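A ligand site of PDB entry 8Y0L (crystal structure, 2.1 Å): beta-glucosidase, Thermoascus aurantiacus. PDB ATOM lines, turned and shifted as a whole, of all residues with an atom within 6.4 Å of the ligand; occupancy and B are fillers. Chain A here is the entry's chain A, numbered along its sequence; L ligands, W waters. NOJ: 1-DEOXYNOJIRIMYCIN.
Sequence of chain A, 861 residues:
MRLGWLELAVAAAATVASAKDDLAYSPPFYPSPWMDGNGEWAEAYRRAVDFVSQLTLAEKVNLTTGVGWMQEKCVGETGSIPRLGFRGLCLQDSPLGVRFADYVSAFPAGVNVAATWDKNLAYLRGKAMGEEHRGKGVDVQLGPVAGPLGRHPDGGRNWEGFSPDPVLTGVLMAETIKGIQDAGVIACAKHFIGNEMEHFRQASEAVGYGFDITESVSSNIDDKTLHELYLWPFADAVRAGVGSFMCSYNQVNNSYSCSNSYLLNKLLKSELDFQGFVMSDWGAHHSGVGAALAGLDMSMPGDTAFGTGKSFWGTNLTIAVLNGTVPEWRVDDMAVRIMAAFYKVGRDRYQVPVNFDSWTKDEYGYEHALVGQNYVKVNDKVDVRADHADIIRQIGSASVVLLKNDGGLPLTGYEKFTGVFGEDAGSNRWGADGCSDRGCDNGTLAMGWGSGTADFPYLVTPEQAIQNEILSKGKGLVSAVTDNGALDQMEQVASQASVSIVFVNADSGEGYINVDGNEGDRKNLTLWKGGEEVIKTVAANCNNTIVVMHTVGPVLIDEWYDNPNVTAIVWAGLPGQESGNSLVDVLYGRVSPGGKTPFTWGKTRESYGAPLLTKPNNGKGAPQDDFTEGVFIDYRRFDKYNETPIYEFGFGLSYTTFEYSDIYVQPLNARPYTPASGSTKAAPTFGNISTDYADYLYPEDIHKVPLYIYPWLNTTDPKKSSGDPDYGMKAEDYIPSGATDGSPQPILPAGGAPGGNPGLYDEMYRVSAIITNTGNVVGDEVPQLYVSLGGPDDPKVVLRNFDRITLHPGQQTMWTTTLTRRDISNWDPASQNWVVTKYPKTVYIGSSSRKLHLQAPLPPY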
ATOM      1  N   TRP A  69      -9.252 -21.083 -26.990  1.00  0.00           N
ATOM      2  CA  TRP A  69      -9.226 -20.317 -25.756  1.00  0.00           C
ATOM      3  C   TRP A  69      -8.470 -21.066 -24.667  1.00  0.00           C
ATOM      4  O   TRP A  69      -8.859 -22.181 -24.290  1.00  0.00           O
ATOM      5  CB  TRP A  69     -10.667 -19.996 -25.305  1.00  0.00           C
ATOM      6  CG  TRP A  69     -10.771 -19.216 -24.021  1.00  0.00           C
ATOM      7  CD1 TRP A  69     -11.528 -19.541 -22.946  1.00  0.00           C
ATOM      8  CD2 TRP A  69     -10.114 -17.970 -23.686  1.00  0.00           C
ATOM      9  NE1 TRP A  69     -11.386 -18.602 -21.955  1.00  0.00           N
ATOM     10  CE2 TRP A  69     -10.534 -17.623 -22.380  1.00  0.00           C
ATOM     11  CE3 TRP A  69      -9.220 -17.119 -24.348  1.00  0.00           C
ATOM     12  CZ2 TRP A  69     -10.091 -16.475 -21.734  1.00  0.00           C
ATOM     13  CZ3 TRP A  69      -8.787 -15.980 -23.707  1.00  0.00           C
ATOM     14  CH2 TRP A  69      -9.214 -15.667 -22.414  1.00  0.00           C
ATOM     15  N   VAL A  75      -2.680 -15.017 -24.400  1.00  0.00           N
ATOM     16  CA  VAL A  75      -4.102 -14.720 -24.506  1.00  0.00           C
ATOM     17  C   VAL A  75      -4.628 -15.251 -25.841  1.00  0.00           C
ATOM     18  O   VAL A  75      -5.729 -15.801 -25.893  1.00  0.00           O
ATOM     19  CB  VAL A  75      -4.380 -13.207 -24.356  1.00  0.00           C
ATOM     20  CG1 VAL A  75      -5.824 -12.843 -24.688  1.00  0.00           C
ATOM     21  CG2 VAL A  75      -4.024 -12.703 -22.963  1.00  0.00           C
ATOM     22  N   ASP A  93      -2.578  -9.191 -24.258  1.00  0.00           N
ATOM     23  CA  ASP A  93      -3.009  -7.936 -23.665  1.00  0.00           C
ATOM     24  C   ASP A  93      -1.840  -7.354 -22.864  1.00  0.00           C
ATOM     25  O   ASP A  93      -0.957  -8.101 -22.473  1.00  0.00           O
ATOM     26  CB  ASP A  93      -4.238  -8.157 -22.782  1.00  0.00           C
ATOM     27  CG  ASP A  93      -5.514  -8.574 -23.498  1.00  0.00           C
ATOM     28  OD1 ASP A  93      -5.860  -7.933 -24.511  1.00  0.00           O
ATOM     29  OD2 ASP A  93      -6.156  -9.543 -23.034  1.00  0.00           O
ATOM     30  N   ARG A  99      -0.334  -8.199 -19.639  1.00  0.00           N
ATOM     31  CA  ARG A  99      -1.371  -8.774 -18.812  1.00  0.00           C
ATOM     32  C   ARG A  99      -0.941 -10.151 -18.325  1.00  0.00           C
ATOM     33  O   ARG A  99      -0.248 -10.869 -19.041  1.00  0.00           O
ATOM     34  CB  ARG A  99      -2.675  -8.859 -19.617  1.00  0.00           C
ATOM     35  CG  ARG A  99      -3.901  -9.229 -18.786  1.00  0.00           C
ATOM     36  CD  ARG A  99      -5.138  -9.384 -19.645  1.00  0.00           C
ATOM     37  NE  ARG A  99      -6.291  -9.820 -18.846  1.00  0.00           N
ATOM     38  CZ  ARG A  99      -7.438 -10.292 -19.338  1.00  0.00           C
ATOM     39  NH1 ARG A  99      -7.623 -10.378 -20.649  1.00  0.00           N
ATOM     40  NH2 ARG A  99      -8.399 -10.673 -18.512  1.00  0.00           N
ATOM     41  N   PHE A 100      -1.315 -10.485 -17.075  1.00  0.00           N
ATOM     42  CA  PHE A 100      -1.258 -11.841 -16.536  1.00  0.00           C
ATOM     43  C   PHE A 100       0.142 -12.185 -16.031  1.00  0.00           C
ATOM     44  O   PHE A 100       0.276 -12.790 -14.967  1.00  0.00           O
ATOM     45  CB  PHE A 100      -1.752 -12.916 -17.512  1.00  0.00           C
ATOM     46  CG  PHE A 100      -3.262 -12.939 -17.728  1.00  0.00           C
ATOM     47  CD1 PHE A 100      -4.139 -12.893 -16.655  1.00  0.00           C
ATOM     48  CD2 PHE A 100      -3.799 -12.997 -19.017  1.00  0.00           C
ATOM     49  CE1 PHE A 100      -5.512 -12.918 -16.859  1.00  0.00           C
ATOM     50  CE2 PHE A 100      -5.167 -13.025 -19.208  1.00  0.00           C
ATOM     51  CZ  PHE A 100      -6.021 -12.982 -18.137  1.00  0.00           C
ATOM     52  N   LEU A 142      -1.700  -6.336 -27.703  1.00  0.00           N
ATOM     53  CA  LEU A 142      -3.068  -6.038 -28.091  1.00  0.00           C
ATOM     54  C   LEU A 142      -3.460  -4.641 -27.615  1.00  0.00           C
ATOM     55  O   LEU A 142      -4.190  -4.470 -26.644  1.00  0.00           O
ATOM     56  CB  LEU A 142      -3.995  -7.141 -27.578  1.00  0.00           C
ATOM     57  CG  LEU A 142      -3.705  -8.554 -28.110  1.00  0.00           C
ATOM     58  CD1 LEU A 142      -4.653  -9.584 -27.532  1.00  0.00           C
ATOM     59  CD2 LEU A 142      -3.756  -8.602 -29.633  1.00  0.00           C
ATOM     60  N   VAL A 145      -5.458   1.664 -28.042  1.00  0.00           N
ATOM     61  CA  VAL A 145      -6.890   1.767 -28.277  1.00  0.00           C
ATOM     62  C   VAL A 145      -7.245   3.152 -28.794  1.00  0.00           C
ATOM     63  O   VAL A 145      -6.900   4.155 -28.173  1.00  0.00           O
ATOM     64  CB  VAL A 145      -7.655   1.449 -26.968  1.00  0.00           C
ATOM     65  CG1 VAL A 145      -9.149   1.721 -27.082  1.00  0.00           C
ATOM     66  CG2 VAL A 145      -7.405   0.029 -26.495  1.00  0.00           C
ATOM     67  N   ARG A 157     -15.004   1.570 -21.238  1.00  0.00           N
ATOM     68  CA  ARG A 157     -13.627   1.296 -21.611  1.00  0.00           C
ATOM     69  C   ARG A 157     -12.930   2.532 -22.199  1.00  0.00           C
ATOM     70  O   ARG A 157     -11.846   2.400 -22.760  1.00  0.00           O
ATOM     71  CB  ARG A 157     -13.549   0.160 -22.639  1.00  0.00           C
ATOM     72  CG  ARG A 157     -14.168  -1.151 -22.173  1.00  0.00           C
ATOM     73  CD  ARG A 157     -13.951  -2.265 -23.192  1.00  0.00           C
ATOM     74  NE  ARG A 157     -12.541  -2.669 -23.303  1.00  0.00           N
ATOM     75  CZ  ARG A 157     -12.083  -3.670 -24.043  1.00  0.00           C
ATOM     76  NH1 ARG A 157     -12.887  -4.336 -24.845  1.00  0.00           N
ATOM     77  NH2 ARG A 157     -10.795  -3.983 -23.986  1.00  0.00           N
ATOM     78  N   GLU A 160      -9.228   3.216 -21.494  1.00  0.00           N
ATOM     79  CA  GLU A 160      -8.222   2.408 -22.175  1.00  0.00           C
ATOM     80  C   GLU A 160      -7.632   3.168 -23.367  1.00  0.00           C
ATOM     81  O   GLU A 160      -6.484   2.934 -23.735  1.00  0.00           O
ATOM     82  CB  GLU A 160      -8.812   1.102 -22.711  1.00  0.00           C
ATOM     83  CG  GLU A 160      -9.202   0.101 -21.622  1.00  0.00           C
ATOM     84  CD  GLU A 160      -9.194  -1.333 -22.126  1.00  0.00           C
ATOM     85  OE1 GLU A 160      -8.138  -1.725 -22.666  1.00  0.00           O
ATOM     86  OE2 GLU A 160     -10.206  -2.038 -21.993  1.00  0.00           O
ATOM     87  N   LYS A 190      -6.924  -1.274 -31.845  1.00  0.00           N
ATOM     88  CA  LYS A 190      -8.243  -1.816 -31.543  1.00  0.00           C
ATOM     89  C   LYS A 190      -9.094  -0.698 -30.947  1.00  0.00           C
ATOM     90  O   LYS A 190      -8.545   0.325 -30.541  1.00  0.00           O
ATOM     91  CB  LYS A 190      -8.089  -3.012 -30.598  1.00  0.00           C
ATOM     92  CG  LYS A 190      -7.786  -2.691 -29.132  1.00  0.00           C
ATOM     93  CD  LYS A 190      -7.412  -3.940 -28.323  1.00  0.00           C
ATOM     94  CE  LYS A 190      -7.453  -3.737 -26.842  1.00  0.00           C
ATOM     95  NZ  LYS A 190      -6.999  -4.944 -26.144  1.00  0.00           N
ATOM     96  N   HIS A 191     -10.424  -0.844 -30.907  1.00  0.00           N
ATOM     97  CA  HIS A 191     -11.187  -1.867 -31.608  1.00  0.00           C
ATOM     98  C   HIS A 191     -11.869  -1.198 -32.802  1.00  0.00           C
ATOM     99  O   HIS A 191     -12.468  -0.134 -32.656  1.00  0.00           O
ATOM    100  CB  HIS A 191     -12.248  -2.463 -30.681  1.00  0.00           C
ATOM    101  CG  HIS A 191     -11.716  -2.918 -29.364  1.00  0.00           C
ATOM    102  ND1 HIS A 191     -11.496  -2.053 -28.306  1.00  0.00           N
ATOM    103  CD2 HIS A 191     -11.344  -4.136 -28.940  1.00  0.00           C
ATOM    104  CE1 HIS A 191     -11.018  -2.745 -27.275  1.00  0.00           C
ATOM    105  NE2 HIS A 191     -10.911  -4.010 -27.639  1.00  0.00           N
ATOM    106  N   ASN A 195     -17.213   0.627 -31.262  1.00  0.00           N
ATOM    107  CA  ASN A 195     -17.463  -0.048 -30.005  1.00  0.00           C
ATOM    108  C   ASN A 195     -17.431   0.986 -28.874  1.00  0.00           C
ATOM    109  O   ASN A 195     -16.532   0.958 -28.035  1.00  0.00           O
ATOM    110  CB  ASN A 195     -16.455  -1.169 -29.787  1.00  0.00           C
ATOM    111  CG  ASN A 195     -16.757  -2.050 -28.597  1.00  0.00           C
ATOM    112  OD1 ASN A 195     -17.869  -2.024 -28.050  1.00  0.00           O
ATOM    113  ND2 ASN A 195     -15.784  -2.854 -28.187  1.00  0.00           N
ATOM    114  N   GLU A 198     -20.217  -0.749 -23.772  1.00  0.00           N
ATOM    115  CA  GLU A 198     -20.088  -2.159 -23.449  1.00  0.00           C
ATOM    116  C   GLU A 198     -21.433  -2.883 -23.589  1.00  0.00           C
ATOM    117  O   GLU A 198     -21.444  -4.062 -23.937  1.00  0.00           O
ATOM    118  CB  GLU A 198     -19.462  -2.326 -22.064  1.00  0.00           C
ATOM    119  CG  GLU A 198     -17.987  -1.955 -22.064  1.00  0.00           C
ATOM    120  CD  GLU A 198     -17.176  -2.695 -23.119  1.00  0.00           C
ATOM    121  OE1 GLU A 198     -16.860  -3.883 -22.892  1.00  0.00           O
ATOM    122  OE2 GLU A 198     -16.911  -2.095 -24.179  1.00  0.00           O
ATOM    123  N   ARG A 201     -22.551  -5.665 -26.495  1.00  0.00           N
ATOM    124  CA  ARG A 201     -21.433  -5.821 -27.414  1.00  0.00           C
ATOM    125  C   ARG A 201     -21.409  -7.261 -27.941  1.00  0.00           C
ATOM    126  O   ARG A 201     -20.979  -7.497 -29.068  1.00  0.00           O
ATOM    127  CB  ARG A 201     -20.097  -5.452 -26.750  1.00  0.00           C
ATOM    128  CG  ARG A 201     -19.613  -6.430 -25.688  1.00  0.00           C
ATOM    129  CD  ARG A 201     -18.386  -5.892 -24.977  1.00  0.00           C
ATOM    130  NE  ARG A 201     -17.849  -6.874 -24.016  1.00  0.00           N
ATOM    131  CZ  ARG A 201     -16.567  -7.202 -23.866  1.00  0.00           C
ATOM    132  NH1 ARG A 201     -15.622  -6.555 -24.519  1.00  0.00           N
ATOM    133  NH2 ARG A 201     -16.241  -8.157 -23.014  1.00  0.00           N
ATOM    134  N   MET A 246      -7.529  -4.903 -34.872  1.00  0.00           N
ATOM    135  CA  MET A 246      -8.516  -5.810 -34.303  1.00  0.00           C
ATOM    136  C   MET A 246      -9.916  -5.279 -34.590  1.00  0.00           C
ATOM    137  O   MET A 246     -10.265  -4.186 -34.149  1.00  0.00           O
ATOM    138  CB  MET A 246      -8.340  -5.977 -32.790  1.00  0.00           C
ATOM    139  CG  MET A 246      -9.303  -6.960 -32.154  1.00  0.00           C
ATOM    140  SD  MET A 246      -9.250  -6.962 -30.353  1.00  0.00           S
ATOM    141  CE  MET A 246      -7.560  -7.520 -30.077  1.00  0.00           C
ATOM    142  N   TYR A 249     -16.403  -6.271 -31.637  1.00  0.00           N
ATOM    143  CA  TYR A 249     -17.498  -7.195 -31.356  1.00  0.00           C
ATOM    144  C   TYR A 249     -18.804  -6.726 -31.989  1.00  0.00           C
ATOM    145  O   TYR A 249     -19.625  -7.541 -32.403  1.00  0.00           O
ATOM    146  CB  TYR A 249     -17.718  -7.315 -29.837  1.00  0.00           C
ATOM    147  CG  TYR A 249     -16.794  -8.259 -29.086  1.00  0.00           C
ATOM    148  CD1 TYR A 249     -16.698  -9.602 -29.425  1.00  0.00           C
ATOM    149  CD2 TYR A 249     -16.019  -7.810 -28.017  1.00  0.00           C
ATOM    150  CE1 TYR A 249     -15.861 -10.473 -28.737  1.00  0.00           C
ATOM    151  CE2 TYR A 249     -15.175  -8.665 -27.329  1.00  0.00           C
ATOM    152  CZ  TYR A 249     -15.098 -10.000 -27.681  1.00  0.00           C
ATOM    153  OH  TYR A 249     -14.269 -10.836 -26.989  1.00  0.00           O
ATOM    154  N   ASP A 281     -11.634  -9.698 -32.697  1.00  0.00           N
ATOM    155  CA  ASP A 281     -11.735  -9.713 -31.251  1.00  0.00           C
ATOM    156  C   ASP A 281     -12.139 -11.130 -30.854  1.00  0.00           C
ATOM    157  O   ASP A 281     -12.624 -11.904 -31.683  1.00  0.00           O
ATOM    158  CB  ASP A 281     -12.620  -8.596 -30.719  1.00  0.00           C
ATOM    159  CG  ASP A 281     -12.335  -8.177 -29.285  1.00  0.00           C
ATOM    160  OD1 ASP A 281     -11.605  -8.921 -28.609  1.00  0.00           O
ATOM    161  OD2 ASP A 281     -12.820  -7.102 -28.869  1.00  0.00           O
ATOM    162  N   TRP A 282     -11.909 -11.469 -29.578  1.00  0.00           N
ATOM    163  CA  TRP A 282     -11.962 -12.848 -29.123  1.00  0.00           C
ATOM    164  C   TRP A 282     -13.390 -13.391 -29.192  1.00  0.00           C
ATOM    165  O   TRP A 282     -14.217 -13.071 -28.341  1.00  0.00           O
ATOM    166  CB  TRP A 282     -11.403 -12.964 -27.697  1.00  0.00           C
ATOM    167  CG  TRP A 282      -9.929 -13.251 -27.618  1.00  0.00           C
ATOM    168  CD1 TRP A 282      -9.336 -14.118 -26.748  1.00  0.00           C
ATOM    169  CD2 TRP A 282      -8.858 -12.679 -28.414  1.00  0.00           C
ATOM    170  NE1 TRP A 282      -7.981 -14.142 -26.949  1.00  0.00           N
ATOM    171  CE2 TRP A 282      -7.657 -13.263 -27.953  1.00  0.00           C
ATOM    172  CE3 TRP A 282      -8.782 -11.738 -29.447  1.00  0.00           C
ATOM    173  CZ2 TRP A 282      -6.413 -12.943 -28.496  1.00  0.00           C
ATOM    174  CZ3 TRP A 282      -7.555 -11.418 -29.975  1.00  0.00           C
ATOM    175  CH2 TRP A 282      -6.381 -12.010 -29.505  1.00  0.00           C
ATOM    176  N   SER A 451      -9.847  -6.562 -19.659  1.00  0.00           N
ATOM    177  CA  SER A 451      -8.691  -7.060 -20.377  1.00  0.00           C
ATOM    178  C   SER A 451      -7.587  -5.997 -20.424  1.00  0.00           C
ATOM    179  O   SER A 451      -6.418  -6.332 -20.629  1.00  0.00           O
ATOM    180  CB  SER A 451      -9.062  -7.509 -21.767  1.00  0.00           C
ATOM    181  OG  SER A 451      -9.498  -6.404 -22.560  1.00  0.00           O
ATOM    182  N   GLY A 452      -7.970  -4.725 -20.241  1.00  0.00           N
ATOM    183  CA  GLY A 452      -7.029  -3.625 -20.375  1.00  0.00           C
ATOM    184  C   GLY A 452      -6.162  -3.433 -19.131  1.00  0.00           C
ATOM    185  O   GLY A 452      -5.979  -2.302 -18.678  1.00  0.00           O
ATOM    186  N   GLU A 510     -14.422  -3.284 -18.826  1.00  0.00           N
ATOM    187  CA  GLU A 510     -14.987  -4.137 -19.853  1.00  0.00           C
ATOM    188  C   GLU A 510     -16.258  -4.796 -19.324  1.00  0.00           C
ATOM    189  O   GLU A 510     -16.390  -5.040 -18.124  1.00  0.00           O
ATOM    190  CB  GLU A 510     -13.918  -5.144 -20.271  1.00  0.00           C
ATOM    191  CG  GLU A 510     -14.266  -5.930 -21.531  1.00  0.00           C
ATOM    192  CD  GLU A 510     -13.145  -6.802 -22.065  1.00  0.00           C
ATOM    193  OE1 GLU A 510     -13.423  -7.687 -22.898  1.00  0.00           O
ATOM    194  OE2 GLU A 510     -11.979  -6.577 -21.662  1.00  0.00           O
HETATM  195  C1  NOJ L   1     -11.769  -8.983 -25.574  1.00  0.00           C
HETATM  196  C2  NOJ L   1     -11.406  -7.507 -25.539  1.00  0.00           C
HETATM  197  O2  NOJ L   1     -12.474  -6.787 -26.165  1.00  0.00           O
HETATM  198  C3  NOJ L   1     -10.083  -7.230 -26.237  1.00  0.00           C
HETATM  199  O3  NOJ L   1      -9.715  -5.859 -26.056  1.00  0.00           O
HETATM  200  C4  NOJ L   1      -9.005  -8.138 -25.676  1.00  0.00           C
HETATM  201  O4  NOJ L   1      -7.778  -7.940 -26.367  1.00  0.00           O
HETATM  202  C5  NOJ L   1      -9.410  -9.608 -25.825  1.00  0.00           C
HETATM  203  N5  NOJ L   1     -10.676  -9.841 -25.118  1.00  0.00           N
HETATM  204  C6  NOJ L   1      -8.354 -10.579 -25.317  1.00  0.00           C
HETATM  205  O6  NOJ L   1      -8.352 -10.593 -23.890  1.00  0.00           O
HETATM  206  O   HOH W   1     -11.821  -9.892 -22.484  1.00  0.00           O
HETATM  207  O   HOH W   2     -11.687 -12.362 -24.547  1.00  0.00           O
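Water W1 bridges the side-chain carboxylate of Glu 510 (2.8 Å) and a nitrogen (N5) of the ligand (2.9 Å).
Val 75 touches the ligand (CG1 to C6, 3.5 Å).
CD1 of Leu 142 touches O4 of the ligand, 3.7 Å away.
Arg 201 touches the ligand (NH1 to O2, 3.6 Å).
Met 246 touches the ligand.
Tyr 249 touches the ligand.
Trp 282 touches the ligand.
Ser 451 touches the ligand (OG to O3, 3.5 Å).
Glu 510 touches the ligand (OE1 to C2, 3.3 Å).
Hydrophobic or aromatic side chains within 4 Å of the ligand: Val 75, Leu 142, His 191, Met 246, Tyr 249 and Trp 282.
Within 4 Å of the ligand: Val 75, Asp 93, Arg 99, Leu 142, Arg 157, Lys 190, His 191, Arg 201, Met 246, Tyr 249, Asp 281, Trp 282, Ser 451 and Glu 510.
The side-chain carboxylate (OD1) of Asp 93 is in salt-bridge range of the side-chain amino group (NZ) of Lys 190 (3.6 Å).
OD2 of Asp 93 is in salt-bridge range of NH1 of Arg 99, at 2.9 Å.
NH2 of Arg 157 lies within salt-bridge range of OE2 of Glu 510.
NH2 of Arg 157 is in hydrogen-bond range of OG of Ser 451 (3.1 Å).
The backbone carbonyl oxygen (O) of Leu 142 sits at hydrogen-bond distance from the side-chain amino group (NZ) of Lys 190, 2.9 Å away.
OE2 of Glu 510 is in hydrogen-bond range of OG of Ser 451, 2.6 Å away.
OE1 of Glu 510 is in salt-bridge range of NH2 of Arg 201, at 2.9 Å.
OH of Tyr 249 sits at hydrogen-bond distance from O of Trp 282 (2.6 Å).
The side-chain carboxylate (OD2) of Asp 93 lies within hydrogen-bond range of an oxygen (O6) of the ligand, at 2.6 Å.
NE2 of His 191 sits at hydrogen-bond distance from O3 of the ligand, at 2.7 Å.
The side-chain carboxylate (OD1) of Asp 281 lies within salt-bridge range of a nitrogen (N5) of the ligand (3.7 Å).
O2 of the ligand sits at hydrogen-bond distance from NH1 of Arg 157.
The side-chain amino group (NZ) of Lys 190 sits at hydrogen-bond distance from an oxygen (O3) of the ligand.
The guanidinium group (NH1) of Arg 99 is in hydrogen-bond range of an oxygen (O6) of the ligand, at 3.3 Å.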
